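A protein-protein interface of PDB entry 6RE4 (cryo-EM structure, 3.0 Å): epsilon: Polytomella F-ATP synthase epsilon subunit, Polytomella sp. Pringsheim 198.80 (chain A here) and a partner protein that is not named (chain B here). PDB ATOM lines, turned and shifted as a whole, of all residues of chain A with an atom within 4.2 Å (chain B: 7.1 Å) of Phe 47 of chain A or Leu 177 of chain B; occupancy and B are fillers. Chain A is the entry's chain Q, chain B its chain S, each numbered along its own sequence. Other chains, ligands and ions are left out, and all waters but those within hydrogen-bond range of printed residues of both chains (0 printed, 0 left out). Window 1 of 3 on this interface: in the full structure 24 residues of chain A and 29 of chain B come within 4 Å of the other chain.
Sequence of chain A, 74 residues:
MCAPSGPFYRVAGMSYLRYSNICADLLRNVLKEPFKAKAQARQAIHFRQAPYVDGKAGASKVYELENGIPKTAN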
ATOM      1  N   ARG A  18      21.608 -11.432 -26.686  1.00  0.00           N
ATOM      2  CA  ARG A  18      21.161 -10.450 -25.708  1.00  0.00           C
ATOM      3  C   ARG A  18      20.988  -9.076 -26.326  1.00  0.00           C
ATOM      4  O   ARG A  18      20.021  -8.385 -26.001  1.00  0.00           O
ATOM      5  CB  ARG A  18      22.132 -10.370 -24.546  1.00  0.00           C
ATOM      6  CG  ARG A  18      21.565  -9.598 -23.394  1.00  0.00           C
ATOM      7  CD  ARG A  18      22.451  -9.725 -22.205  1.00  0.00           C
ATOM      8  NE  ARG A  18      22.558 -11.106 -21.767  1.00  0.00           N
ATOM      9  CZ  ARG A  18      22.039 -11.557 -20.638  1.00  0.00           C
ATOM     10  NH1 ARG A  18      21.377 -10.736 -19.842  1.00  0.00           N
ATOM     11  NH2 ARG A  18      22.189 -12.828 -20.310  1.00  0.00           N
ATOM     12  N   ILE A  45       9.982 -14.170 -19.599  1.00  0.00           N
ATOM     13  CA  ILE A  45      10.963 -15.237 -19.465  1.00  0.00           C
ATOM     14  C   ILE A  45      10.704 -15.931 -18.142  1.00  0.00           C
ATOM     15  O   ILE A  45      10.676 -15.276 -17.095  1.00  0.00           O
ATOM     16  CB  ILE A  45      12.399 -14.702 -19.515  1.00  0.00           C
ATOM     17  CG1 ILE A  45      12.627 -13.901 -20.788  1.00  0.00           C
ATOM     18  CG2 ILE A  45      13.382 -15.830 -19.423  1.00  0.00           C
ATOM     19  CD1 ILE A  45      13.939 -13.195 -20.815  1.00  0.00           C
ATOM     20  N   HIS A  46      10.505 -17.247 -18.181  1.00  0.00           N
ATOM     21  CA  HIS A  46      10.228 -18.024 -16.974  1.00  0.00           C
ATOM     22  C   HIS A  46      10.874 -19.393 -17.125  1.00  0.00           C
ATOM     23  O   HIS A  46      10.339 -20.243 -17.834  1.00  0.00           O
ATOM     24  CB  HIS A  46       8.734 -18.179 -16.735  1.00  0.00           C
ATOM     25  CG  HIS A  46       8.023 -16.904 -16.428  1.00  0.00           C
ATOM     26  ND1 HIS A  46       7.533 -16.073 -17.411  1.00  0.00           N
ATOM     27  CD2 HIS A  46       7.689 -16.331 -15.250  1.00  0.00           C
ATOM     28  CE1 HIS A  46       6.937 -15.038 -16.851  1.00  0.00           C
ATOM     29  NE2 HIS A  46       7.020 -15.169 -15.541  1.00  0.00           N
ATOM     30  N   PHE A  47      11.989 -19.607 -16.439  1.00  0.00           N
ATOM     31  CA  PHE A  47      12.614 -20.922 -16.340  1.00  0.00           C
ATOM     32  C   PHE A  47      13.566 -20.902 -15.154  1.00  0.00           C
ATOM     33  O   PHE A  47      13.655 -19.912 -14.423  1.00  0.00           O
ATOM     34  CB  PHE A  47      13.327 -21.325 -17.637  1.00  0.00           C
ATOM     35  CG  PHE A  47      14.580 -20.561 -17.917  1.00  0.00           C
ATOM     36  CD1 PHE A  47      14.528 -19.261 -18.387  1.00  0.00           C
ATOM     37  CD2 PHE A  47      15.813 -21.154 -17.746  1.00  0.00           C
ATOM     38  CE1 PHE A  47      15.671 -18.568 -18.646  1.00  0.00           C
ATOM     39  CE2 PHE A  47      16.964 -20.464 -18.013  1.00  0.00           C
ATOM     40  CZ  PHE A  47      16.891 -19.174 -18.463  1.00  0.00           C
ATOM     41  N   ARG A  48      14.271 -22.009 -14.958  1.00  0.00           N
ATOM     42  CA  ARG A  48      15.294 -22.099 -13.931  1.00  0.00           C
ATOM     43  C   ARG A  48      16.378 -23.055 -14.390  1.00  0.00           C
ATOM     44  O   ARG A  48      16.108 -24.045 -15.068  1.00  0.00           O
ATOM     45  CB  ARG A  48      14.722 -22.565 -12.594  1.00  0.00           C
ATOM     46  CG  ARG A  48      13.859 -23.795 -12.697  1.00  0.00           C
ATOM     47  CD  ARG A  48      13.627 -24.441 -11.353  1.00  0.00           C
ATOM     48  NE  ARG A  48      12.758 -25.607 -11.466  1.00  0.00           N
ATOM     49  CZ  ARG A  48      13.192 -26.841 -11.692  1.00  0.00           C
ATOM     50  NH1 ARG A  48      12.332 -27.842 -11.783  1.00  0.00           N
ATOM     51  NH2 ARG A  48      14.486 -27.075 -11.818  1.00  0.00           N
ATOM     52  N   LYS A  61      18.863 -20.774 -10.523  1.00  0.00           N
ATOM     53  CA  LYS A  61      18.707 -19.392 -10.960  1.00  0.00           C
ATOM     54  C   LYS A  61      17.352 -19.289 -11.643  1.00  0.00           C
ATOM     55  O   LYS A  61      17.224 -19.599 -12.828  1.00  0.00           O
ATOM     56  CB  LYS A  61      19.836 -18.970 -11.894  1.00  0.00           C
ATOM     57  CG  LYS A  61      19.739 -17.526 -12.361  1.00  0.00           C
ATOM     58  CD  LYS A  61      19.653 -16.601 -11.171  1.00  0.00           C
ATOM     59  CE  LYS A  61      19.303 -15.192 -11.569  1.00  0.00           C
ATOM     60  NZ  LYS A  61      19.203 -14.322 -10.367  1.00  0.00           N
ATOM     61  N   VAL A  62      16.353 -18.849 -10.903  1.00  0.00           N
ATOM     62  CA  VAL A  62      14.988 -18.767 -11.396  1.00  0.00           C
ATOM     63  C   VAL A  62      14.770 -17.398 -12.014  1.00  0.00           C
ATOM     64  O   VAL A  62      15.142 -16.372 -11.433  1.00  0.00           O
ATOM     65  CB  VAL A  62      13.987 -19.032 -10.259  1.00  0.00           C
ATOM     66  CG1 VAL A  62      12.564 -19.084 -10.788  1.00  0.00           C
ATOM     67  CG2 VAL A  62      14.352 -20.321  -9.549  1.00  0.00           C
ATOM     68  N   TYR A  63      14.170 -17.380 -13.198  1.00  0.00           N
ATOM     69  CA  TYR A  63      13.864 -16.155 -13.924  1.00  0.00           C
ATOM     70  C   TYR A  63      12.364 -15.923 -13.878  1.00  0.00           C
ATOM     71  O   TYR A  63      11.587 -16.828 -14.184  1.00  0.00           O
ATOM     72  CB  TYR A  63      14.346 -16.245 -15.370  1.00  0.00           C
ATOM     73  CG  TYR A  63      15.847 -16.312 -15.516  1.00  0.00           C
ATOM     74  CD1 TYR A  63      16.526 -17.514 -15.379  1.00  0.00           C
ATOM     75  CD2 TYR A  63      16.586 -15.175 -15.798  1.00  0.00           C
ATOM     76  CE1 TYR A  63      17.893 -17.578 -15.511  1.00  0.00           C
ATOM     77  CE2 TYR A  63      17.951 -15.232 -15.932  1.00  0.00           C
ATOM     78  CZ  TYR A  63      18.596 -16.436 -15.789  1.00  0.00           C
ATOM     79  OH  TYR A  63      19.959 -16.507 -15.921  1.00  0.00           O
ATOM     80  N   ILE A  69      14.654  -9.367 -21.427  1.00  0.00           N
ATOM     81  CA  ILE A  69      15.939  -9.967 -21.079  1.00  0.00           C
ATOM     82  C   ILE A  69      16.609  -8.976 -20.126  1.00  0.00           C
ATOM     83  O   ILE A  69      16.241  -7.790 -20.140  1.00  0.00           O
ATOM     84  CB  ILE A  69      16.749 -10.272 -22.360  1.00  0.00           C
ATOM     85  CG1 ILE A  69      17.383 -11.666 -22.299  1.00  0.00           C
ATOM     86  CG2 ILE A  69      17.829  -9.224 -22.614  1.00  0.00           C
ATOM     87  CD1 ILE A  69      17.892 -12.182 -23.606  1.00  0.00           C
ATOM     88  N   PRO A  70      17.528  -9.390 -19.247  1.00  0.00           N
ATOM     89  CA  PRO A  70      18.151  -8.422 -18.329  1.00  0.00           C
ATOM     90  C   PRO A  70      19.086  -7.476 -19.066  1.00  0.00           C
ATOM     91  O   PRO A  70      20.060  -7.904 -19.686  1.00  0.00           O
ATOM     92  CB  PRO A  70      18.922  -9.309 -17.345  1.00  0.00           C
ATOM     93  CG  PRO A  70      18.331 -10.637 -17.474  1.00  0.00           C
ATOM     94  CD  PRO A  70      17.893 -10.766 -18.879  1.00  0.00           C
ATOM     95  N   ALA B 161      20.766 -28.346 -15.762  1.00  0.00           N
ATOM     96  CA  ALA B 161      19.370 -28.744 -15.867  1.00  0.00           C
ATOM     97  C   ALA B 161      18.514 -27.500 -15.993  1.00  0.00           C
ATOM     98  O   ALA B 161      18.349 -26.761 -15.018  1.00  0.00           O
ATOM     99  CB  ALA B 161      18.936 -29.559 -14.651  1.00  0.00           C
ATOM    100  N   ILE B 162      17.962 -27.272 -17.176  1.00  0.00           N
ATOM    101  CA  ILE B 162      16.989 -26.211 -17.390  1.00  0.00           C
ATOM    102  C   ILE B 162      15.614 -26.827 -17.214  1.00  0.00           C
ATOM    103  O   ILE B 162      15.341 -27.901 -17.755  1.00  0.00           O
ATOM    104  CB  ILE B 162      17.139 -25.572 -18.781  1.00  0.00           C
ATOM    105  CG1 ILE B 162      18.515 -24.927 -18.942  1.00  0.00           C
ATOM    106  CG2 ILE B 162      16.083 -24.514 -19.005  1.00  0.00           C
ATOM    107  CD1 ILE B 162      19.467 -25.717 -19.765  1.00  0.00           C
ATOM    108  N   ALA B 163      14.757 -26.178 -16.437  1.00  0.00           N
ATOM    109  CA  ALA B 163      13.413 -26.688 -16.250  1.00  0.00           C
ATOM    110  C   ALA B 163      12.474 -25.526 -15.994  1.00  0.00           C
ATOM    111  O   ALA B 163      12.881 -24.361 -16.014  1.00  0.00           O
ATOM    112  CB  ALA B 163      13.361 -27.701 -15.115  1.00  0.00           C
ATOM    113  N   ASP B 164      11.205 -25.868 -15.762  1.00  0.00           N
ATOM    114  CA  ASP B 164      10.095 -24.925 -15.609  1.00  0.00           C
ATOM    115  C   ASP B 164       9.955 -24.018 -16.825  1.00  0.00           C
ATOM    116  O   ASP B 164       9.550 -22.863 -16.716  1.00  0.00           O
ATOM    117  CB  ASP B 164      10.210 -24.090 -14.329  1.00  0.00           C
ATOM    118  CG  ASP B 164       9.844 -24.868 -13.084  1.00  0.00           C
ATOM    119  OD1 ASP B 164       9.113 -25.873 -13.202  1.00  0.00           O
ATOM    120  OD2 ASP B 164      10.280 -24.463 -11.984  1.00  0.00           O
ATOM    121  N   THR B 165      10.270 -24.556 -17.997  1.00  0.00           N
ATOM    122  CA  THR B 165      10.260 -23.755 -19.212  1.00  0.00           C
ATOM    123  C   THR B 165       8.844 -23.497 -19.700  1.00  0.00           C
ATOM    124  O   THR B 165       8.473 -22.352 -19.974  1.00  0.00           O
ATOM    125  CB  THR B 165      11.071 -24.464 -20.291  1.00  0.00           C
ATOM    126  OG1 THR B 165      12.425 -24.601 -19.865  1.00  0.00           O
ATOM    127  CG2 THR B 165      11.051 -23.677 -21.530  1.00  0.00           C
ATOM    128  N   TYR B 166       8.032 -24.547 -19.766  1.00  0.00           N
ATOM    129  CA  TYR B 166       6.717 -24.506 -20.381  1.00  0.00           C
ATOM    130  C   TYR B 166       5.624 -24.054 -19.427  1.00  0.00           C
ATOM    131  O   TYR B 166       4.443 -24.250 -19.727  1.00  0.00           O
ATOM    132  CB  TYR B 166       6.366 -25.884 -20.939  1.00  0.00           C
ATOM    133  CG  TYR B 166       7.505 -26.613 -21.612  1.00  0.00           C
ATOM    134  CD1 TYR B 166       7.792 -26.396 -22.940  1.00  0.00           C
ATOM    135  CD2 TYR B 166       8.281 -27.536 -20.920  1.00  0.00           C
ATOM    136  CE1 TYR B 166       8.818 -27.064 -23.563  1.00  0.00           C
ATOM    137  CE2 TYR B 166       9.318 -28.203 -21.539  1.00  0.00           C
ATOM    138  CZ  TYR B 166       9.572 -27.964 -22.861  1.00  0.00           C
ATOM    139  OH  TYR B 166      10.589 -28.624 -23.495  1.00  0.00           O
ATOM    140  N   LYS B 167       5.985 -23.446 -18.297  1.00  0.00           N
ATOM    141  CA  LYS B 167       4.998 -23.101 -17.281  1.00  0.00           C
ATOM    142  C   LYS B 167       4.124 -21.944 -17.736  1.00  0.00           C
ATOM    143  O   LYS B 167       2.892 -22.033 -17.704  1.00  0.00           O
ATOM    144  CB  LYS B 167       5.693 -22.750 -15.968  1.00  0.00           C
ATOM    145  CG  LYS B 167       6.629 -23.802 -15.464  1.00  0.00           C
ATOM    146  CD  LYS B 167       5.933 -25.100 -15.187  1.00  0.00           C
ATOM    147  CE  LYS B 167       5.323 -25.082 -13.805  1.00  0.00           C
ATOM    148  NZ  LYS B 167       6.364 -25.179 -12.749  1.00  0.00           N
ATOM    149  N   PHE B 172      11.339 -16.381 -27.232  1.00  0.00           N
ATOM    150  CA  PHE B 172      12.678 -16.370 -27.796  1.00  0.00           C
ATOM    151  C   PHE B 172      13.699 -15.728 -26.875  1.00  0.00           C
ATOM    152  O   PHE B 172      14.881 -16.063 -26.957  1.00  0.00           O
ATOM    153  CB  PHE B 172      12.702 -15.653 -29.140  1.00  0.00           C
ATOM    154  CG  PHE B 172      13.950 -15.904 -29.902  1.00  0.00           C
ATOM    155  CD1 PHE B 172      14.955 -14.968 -29.938  1.00  0.00           C
ATOM    156  CD2 PHE B 172      14.138 -17.100 -30.544  1.00  0.00           C
ATOM    157  CE1 PHE B 172      16.110 -15.222 -30.615  1.00  0.00           C
ATOM    158  CE2 PHE B 172      15.290 -17.350 -31.218  1.00  0.00           C
ATOM    159  CZ  PHE B 172      16.273 -16.408 -31.258  1.00  0.00           C
ATOM    160  N   GLY B 173      13.278 -14.806 -26.010  1.00  0.00           N
ATOM    161  CA  GLY B 173      14.181 -14.310 -24.990  1.00  0.00           C
ATOM    162  C   GLY B 173      14.580 -15.399 -24.021  1.00  0.00           C
ATOM    163  O   GLY B 173      15.729 -15.464 -23.580  1.00  0.00           O
ATOM    164  N   GLN B 174      13.655 -16.305 -23.727  1.00  0.00           N
ATOM    165  CA  GLN B 174      13.957 -17.429 -22.857  1.00  0.00           C
ATOM    166  C   GLN B 174      14.895 -18.420 -23.534  1.00  0.00           C
ATOM    167  O   GLN B 174      15.862 -18.882 -22.922  1.00  0.00           O
ATOM    168  CB  GLN B 174      12.651 -18.086 -22.446  1.00  0.00           C
ATOM    169  CG  GLN B 174      12.762 -19.385 -21.733  1.00  0.00           C
ATOM    170  CD  GLN B 174      11.426 -20.033 -21.670  1.00  0.00           C
ATOM    171  OE1 GLN B 174      10.968 -20.603 -22.646  1.00  0.00           O
ATOM    172  NE2 GLN B 174      10.746 -19.883 -20.545  1.00  0.00           N
ATOM    173  N   ALA B 175      14.641 -18.731 -24.806  1.00  0.00           N
ATOM    174  CA  ALA B 175      15.519 -19.633 -25.538  1.00  0.00           C
ATOM    175  C   ALA B 175      16.895 -19.028 -25.744  1.00  0.00           C
ATOM    176  O   ALA B 175      17.900 -19.743 -25.724  1.00  0.00           O
ATOM    177  CB  ALA B 175      14.899 -19.992 -26.880  1.00  0.00           C
ATOM    178  N   SER B 176      16.972 -17.706 -25.886  1.00  0.00           N
ATOM    179  CA  SER B 176      18.264 -17.061 -26.053  1.00  0.00           C
ATOM    180  C   SER B 176      19.018 -16.977 -24.738  1.00  0.00           C
ATOM    181  O   SER B 176      20.250 -17.031 -24.725  1.00  0.00           O
ATOM    182  CB  SER B 176      18.081 -15.678 -26.643  1.00  0.00           C
ATOM    183  OG  SER B 176      17.428 -14.845 -25.717  1.00  0.00           O
ATOM    184  N   LEU B 177      18.303 -16.844 -23.619  1.00  0.00           N
ATOM    185  CA  LEU B 177      18.966 -16.917 -22.320  1.00  0.00           C
ATOM    186  C   LEU B 177      19.526 -18.307 -22.066  1.00  0.00           C
ATOM    187  O   LEU B 177      20.650 -18.446 -21.564  1.00  0.00           O
ATOM    188  CB  LEU B 177      17.998 -16.521 -21.218  1.00  0.00           C
ATOM    189  CG  LEU B 177      18.202 -15.106 -20.700  1.00  0.00           C
ATOM    190  CD1 LEU B 177      17.144 -14.752 -19.690  1.00  0.00           C
ATOM    191  CD2 LEU B 177      19.569 -15.002 -20.077  1.00  0.00           C
ATOM    192  N   ILE B 178      18.772 -19.344 -22.448  1.00  0.00           N
ATOM    193  CA  ILE B 178      19.274 -20.715 -22.375  1.00  0.00           C
ATOM    194  C   ILE B 178      20.482 -20.889 -23.285  1.00  0.00           C
ATOM    195  O   ILE B 178      21.465 -21.541 -22.916  1.00  0.00           O
ATOM    196  CB  ILE B 178      18.154 -21.713 -22.719  1.00  0.00           C
ATOM    197  CG1 ILE B 178      17.034 -21.606 -21.699  1.00  0.00           C
ATOM    198  CG2 ILE B 178      18.653 -23.125 -22.672  1.00  0.00           C
ATOM    199  CD1 ILE B 178      15.768 -22.260 -22.131  1.00  0.00           C
ATOM    200  N   VAL B 179      20.458 -20.247 -24.456  1.00  0.00           N
ATOM    201  CA  VAL B 179      21.584 -20.332 -25.378  1.00  0.00           C
ATOM    202  C   VAL B 179      22.827 -19.660 -24.818  1.00  0.00           C
ATOM    203  O   VAL B 179      23.929 -20.189 -24.965  1.00  0.00           O
ATOM    204  CB  VAL B 179      21.213 -19.714 -26.717  1.00  0.00           C
ATOM    205  N   GLU B 180      22.673 -18.504 -24.170  1.00  0.00           N
ATOM    206  CA  GLU B 180      23.823 -17.833 -23.566  1.00  0.00           C
ATOM    207  C   GLU B 180      24.406 -18.658 -22.433  1.00  0.00           C
ATOM    208  O   GLU B 180      25.631 -18.737 -22.275  1.00  0.00           O
ATOM    209  CB  GLU B 180      23.430 -16.463 -23.039  1.00  0.00           C
ATOM    210  CG  GLU B 180      23.120 -15.460 -24.091  1.00  0.00           C
ATOM    211  CD  GLU B 180      22.635 -14.176 -23.485  1.00  0.00           C
ATOM    212  OE1 GLU B 180      23.237 -13.739 -22.485  1.00  0.00           O
ATOM    213  OE2 GLU B 180      21.648 -13.613 -23.995  1.00  0.00           O
ATOM    214  N   GLU B 181      23.545 -19.308 -21.654  1.00  0.00           N
ATOM    215  CA  GLU B 181      24.064 -20.195 -20.625  1.00  0.00           C
ATOM    216  C   GLU B 181      24.674 -21.459 -21.212  1.00  0.00           C
ATOM    217  O   GLU B 181      25.438 -22.133 -20.521  1.00  0.00           O
ATOM    218  CB  GLU B 181      22.959 -20.550 -19.638  1.00  0.00           C
ATOM    219  CG  GLU B 181      22.326 -19.332 -18.961  1.00  0.00           C
ATOM    220  CD  GLU B 181      23.270 -18.553 -18.067  1.00  0.00           C
ATOM    221  OE1 GLU B 181      24.173 -19.164 -17.453  1.00  0.00           O
ATOM    222  OE2 GLU B 181      23.101 -17.322 -17.975  1.00  0.00           O
ATOM    223  N   LEU B 182      24.352 -21.796 -22.460  1.00  0.00           N
ATOM    224  CA  LEU B 182      25.072 -22.868 -23.141  1.00  0.00           C
ATOM    225  C   LEU B 182      26.432 -22.411 -23.645  1.00  0.00           C
ATOM    226  O   LEU B 182      27.389 -23.189 -23.615  1.00  0.00           O
ATOM    227  CB  LEU B 182      24.253 -23.407 -24.309  1.00  0.00           C
ATOM    228  CG  LEU B 182      23.028 -24.229 -23.943  1.00  0.00           C
ATOM    229  CD1 LEU B 182      22.380 -24.783 -25.188  1.00  0.00           C
ATOM    230  CD2 LEU B 182      23.413 -25.327 -22.992  1.00  0.00           C
ATOM    231  N   ILE B 183      26.540 -21.163 -24.115  1.00  0.00           N
ATOM    232  CA  ILE B 183      27.838 -20.627 -24.527  1.00  0.00           C
ATOM    233  C   ILE B 183      28.619 -20.072 -23.340  1.00  0.00           C
ATOM    234  O   ILE B 183      29.671 -19.447 -23.523  1.00  0.00           O
ATOM    235  CB  ILE B 183      27.674 -19.597 -25.667  1.00  0.00           C
ATOM    236  CG1 ILE B 183      26.615 -20.066 -26.645  1.00  0.00           C
ATOM    237  CG2 ILE B 183      28.906 -19.551 -26.572  1.00  0.00           C
ATOM    238  CD1 ILE B 183      26.165 -19.025 -27.618  1.00  0.00           C
ATOM    239  N   LEU B 255      16.962 -23.757 -30.768  1.00  0.00           N
ATOM    240  CA  LEU B 255      16.550 -24.124 -29.428  1.00  0.00           C
ATOM    241  C   LEU B 255      15.102 -23.737 -29.186  1.00  0.00           C
ATOM    242  O   LEU B 255      14.343 -24.503 -28.587  1.00  0.00           O
ATOM    243  CB  LEU B 255      17.477 -23.450 -28.435  1.00  0.00           C
ATOM    244  CG  LEU B 255      17.587 -23.971 -27.034  1.00  0.00           C
ATOM    245  CD1 LEU B 255      18.074 -25.378 -27.117  1.00  0.00           C
ATOM    246  CD2 LEU B 255      18.610 -23.119 -26.379  1.00  0.00           C
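Among the printed residues, pairs that only touch across the chains: Arg 48 of chain A with Ile 162 of chain B (3.3 Å), Arg 18 of chain A with Leu 177 of chain B (3.4 Å), Ile 69 of chain A with Ser 176 of chain B (3.4 Å), Phe 47 of chain A with Ala 163 of chain B (3.5 Å), Arg 48 of chain A with Ala 161 of chain B (3.5 Å), His 46 of chain A with Thr 165 of chain B (3.5 Å), Phe 47 of chain A with Ile 162 of chain B (3.6 Å), Phe 47 of chain A with Asp 164 of chain B (3.6 Å), Ile 45 of chain A with Leu 177 of chain B (3.7 Å), Phe 47 of chain A with Gln 174 of chain B (3.8 Å), Ile 45 of chain A with Gln 174 of chain B (3.8 Å), Tyr 63 of chain A with Glu 181 of chain B (3.8 Å), Phe 47 of chain A with Ile 178 of chain B (3.9 Å), Tyr 63 of chain A with Leu 177 of chain B (3.9 Å), Ile 69 of chain A with Leu 177 of chain B (3.9 Å), Ile 69 of chain A with Gly 173 of chain B (3.9 Å), Ile 45 of chain A with Gly 173 of chain B (3.9 Å) and Phe 47 of chain A with Leu 177 of chain B (3.98 Å).
The guanidinium group (NH1) of Arg 18 of chain A is in hydrogen-bond range of the backbone carbonyl oxygen (O) of Pro 70 of chain A, at 3.1 Å. O of Phe 47 of chain A sits at hydrogen-bond distance from N of Tyr 63 of chain A. The side-chain carboxylate (OD1) of Asp 164 of chain B lies within salt-bridge range of the side-chain amino group (NZ) of Lys 167 of chain B, at 2.9 Å. NE2 of Gln 174 of chain B lies within hydrogen-bond range of O of Thr 165 of chain B. The side-chain hydroxyl (OG) of Ser 176 of chain B sits at hydrogen-bond distance from the backbone carbonyl oxygen (O) of Phe 172 of chain B, 3.1 Å away. OG of Ser 176 of chain B lies within hydrogen-bond range of O of Gly 173 of chain B, at 2.8 Å.
Of the 20 printed residues of chain B, 12 touch a printed residue of chain A. Hydrophobic or aromatic side chains of chain B within 4 Å of the printed part of chain A: Ile 162, Ala 163, Leu 177 and Ile 178. Among the printed residues, 23 pairs touch across the chains. Among the printed residues, Asp or Glu carboxylates within 4 Å of a Lys or Arg side-chain nitrogen of the other chain: Arg 18 of chain A with Glu 180 of chain B and Arg 48 of chain A with Asp 164 of chain B.
The guanidinium group (NH2) of Arg 18 of chain A lies within salt-bridge range of the side-chain carboxylate (OE1) of Glu 180 of chain B (2.6 Å). The backbone carbonyl oxygen (O) of His 46 of chain A sits at hydrogen-bond distance from the side-chain amide nitrogen (NE2) of Gln 174 of chain B (2.8 Å). The backbone NH (N) of Ala 163 of chain B sits at hydrogen-bond distance from the backbone carbonyl oxygen (O) of Arg 48 of chain A (2.9 Å). The guanidinium group of Arg 48 of chain A lies within salt-bridge range of the side-chain carboxylate of Asp 164 of chain B, 2.8 Å away. The backbone carbonyl oxygen (O) of His 46 of chain A lies close to the backbone carbonyl oxygen (O) of Asp 164 of chain B (3.0 Å).
Of the printed residues of chain B, Phe 47 of chain A touches Ile 162 (3.6 Å), Ala 163 (3.5 Å), Asp 164 (3.6 Å), Gln 174 (3.8 Å), Leu 177 (3.98 Å) and Ile 178 (3.9 Å). Printed residues of chain A within 4 Å of Glu 180 of chain B: Arg 18 (2.6 Å). Of the printed residues of chain A, Ile 178 of chain B touches Phe 47. Of the printed residues of chain A, Ser 176 of chain B touches Ile 69. Val 62 of chain A touches none of the printed residues of chain B.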
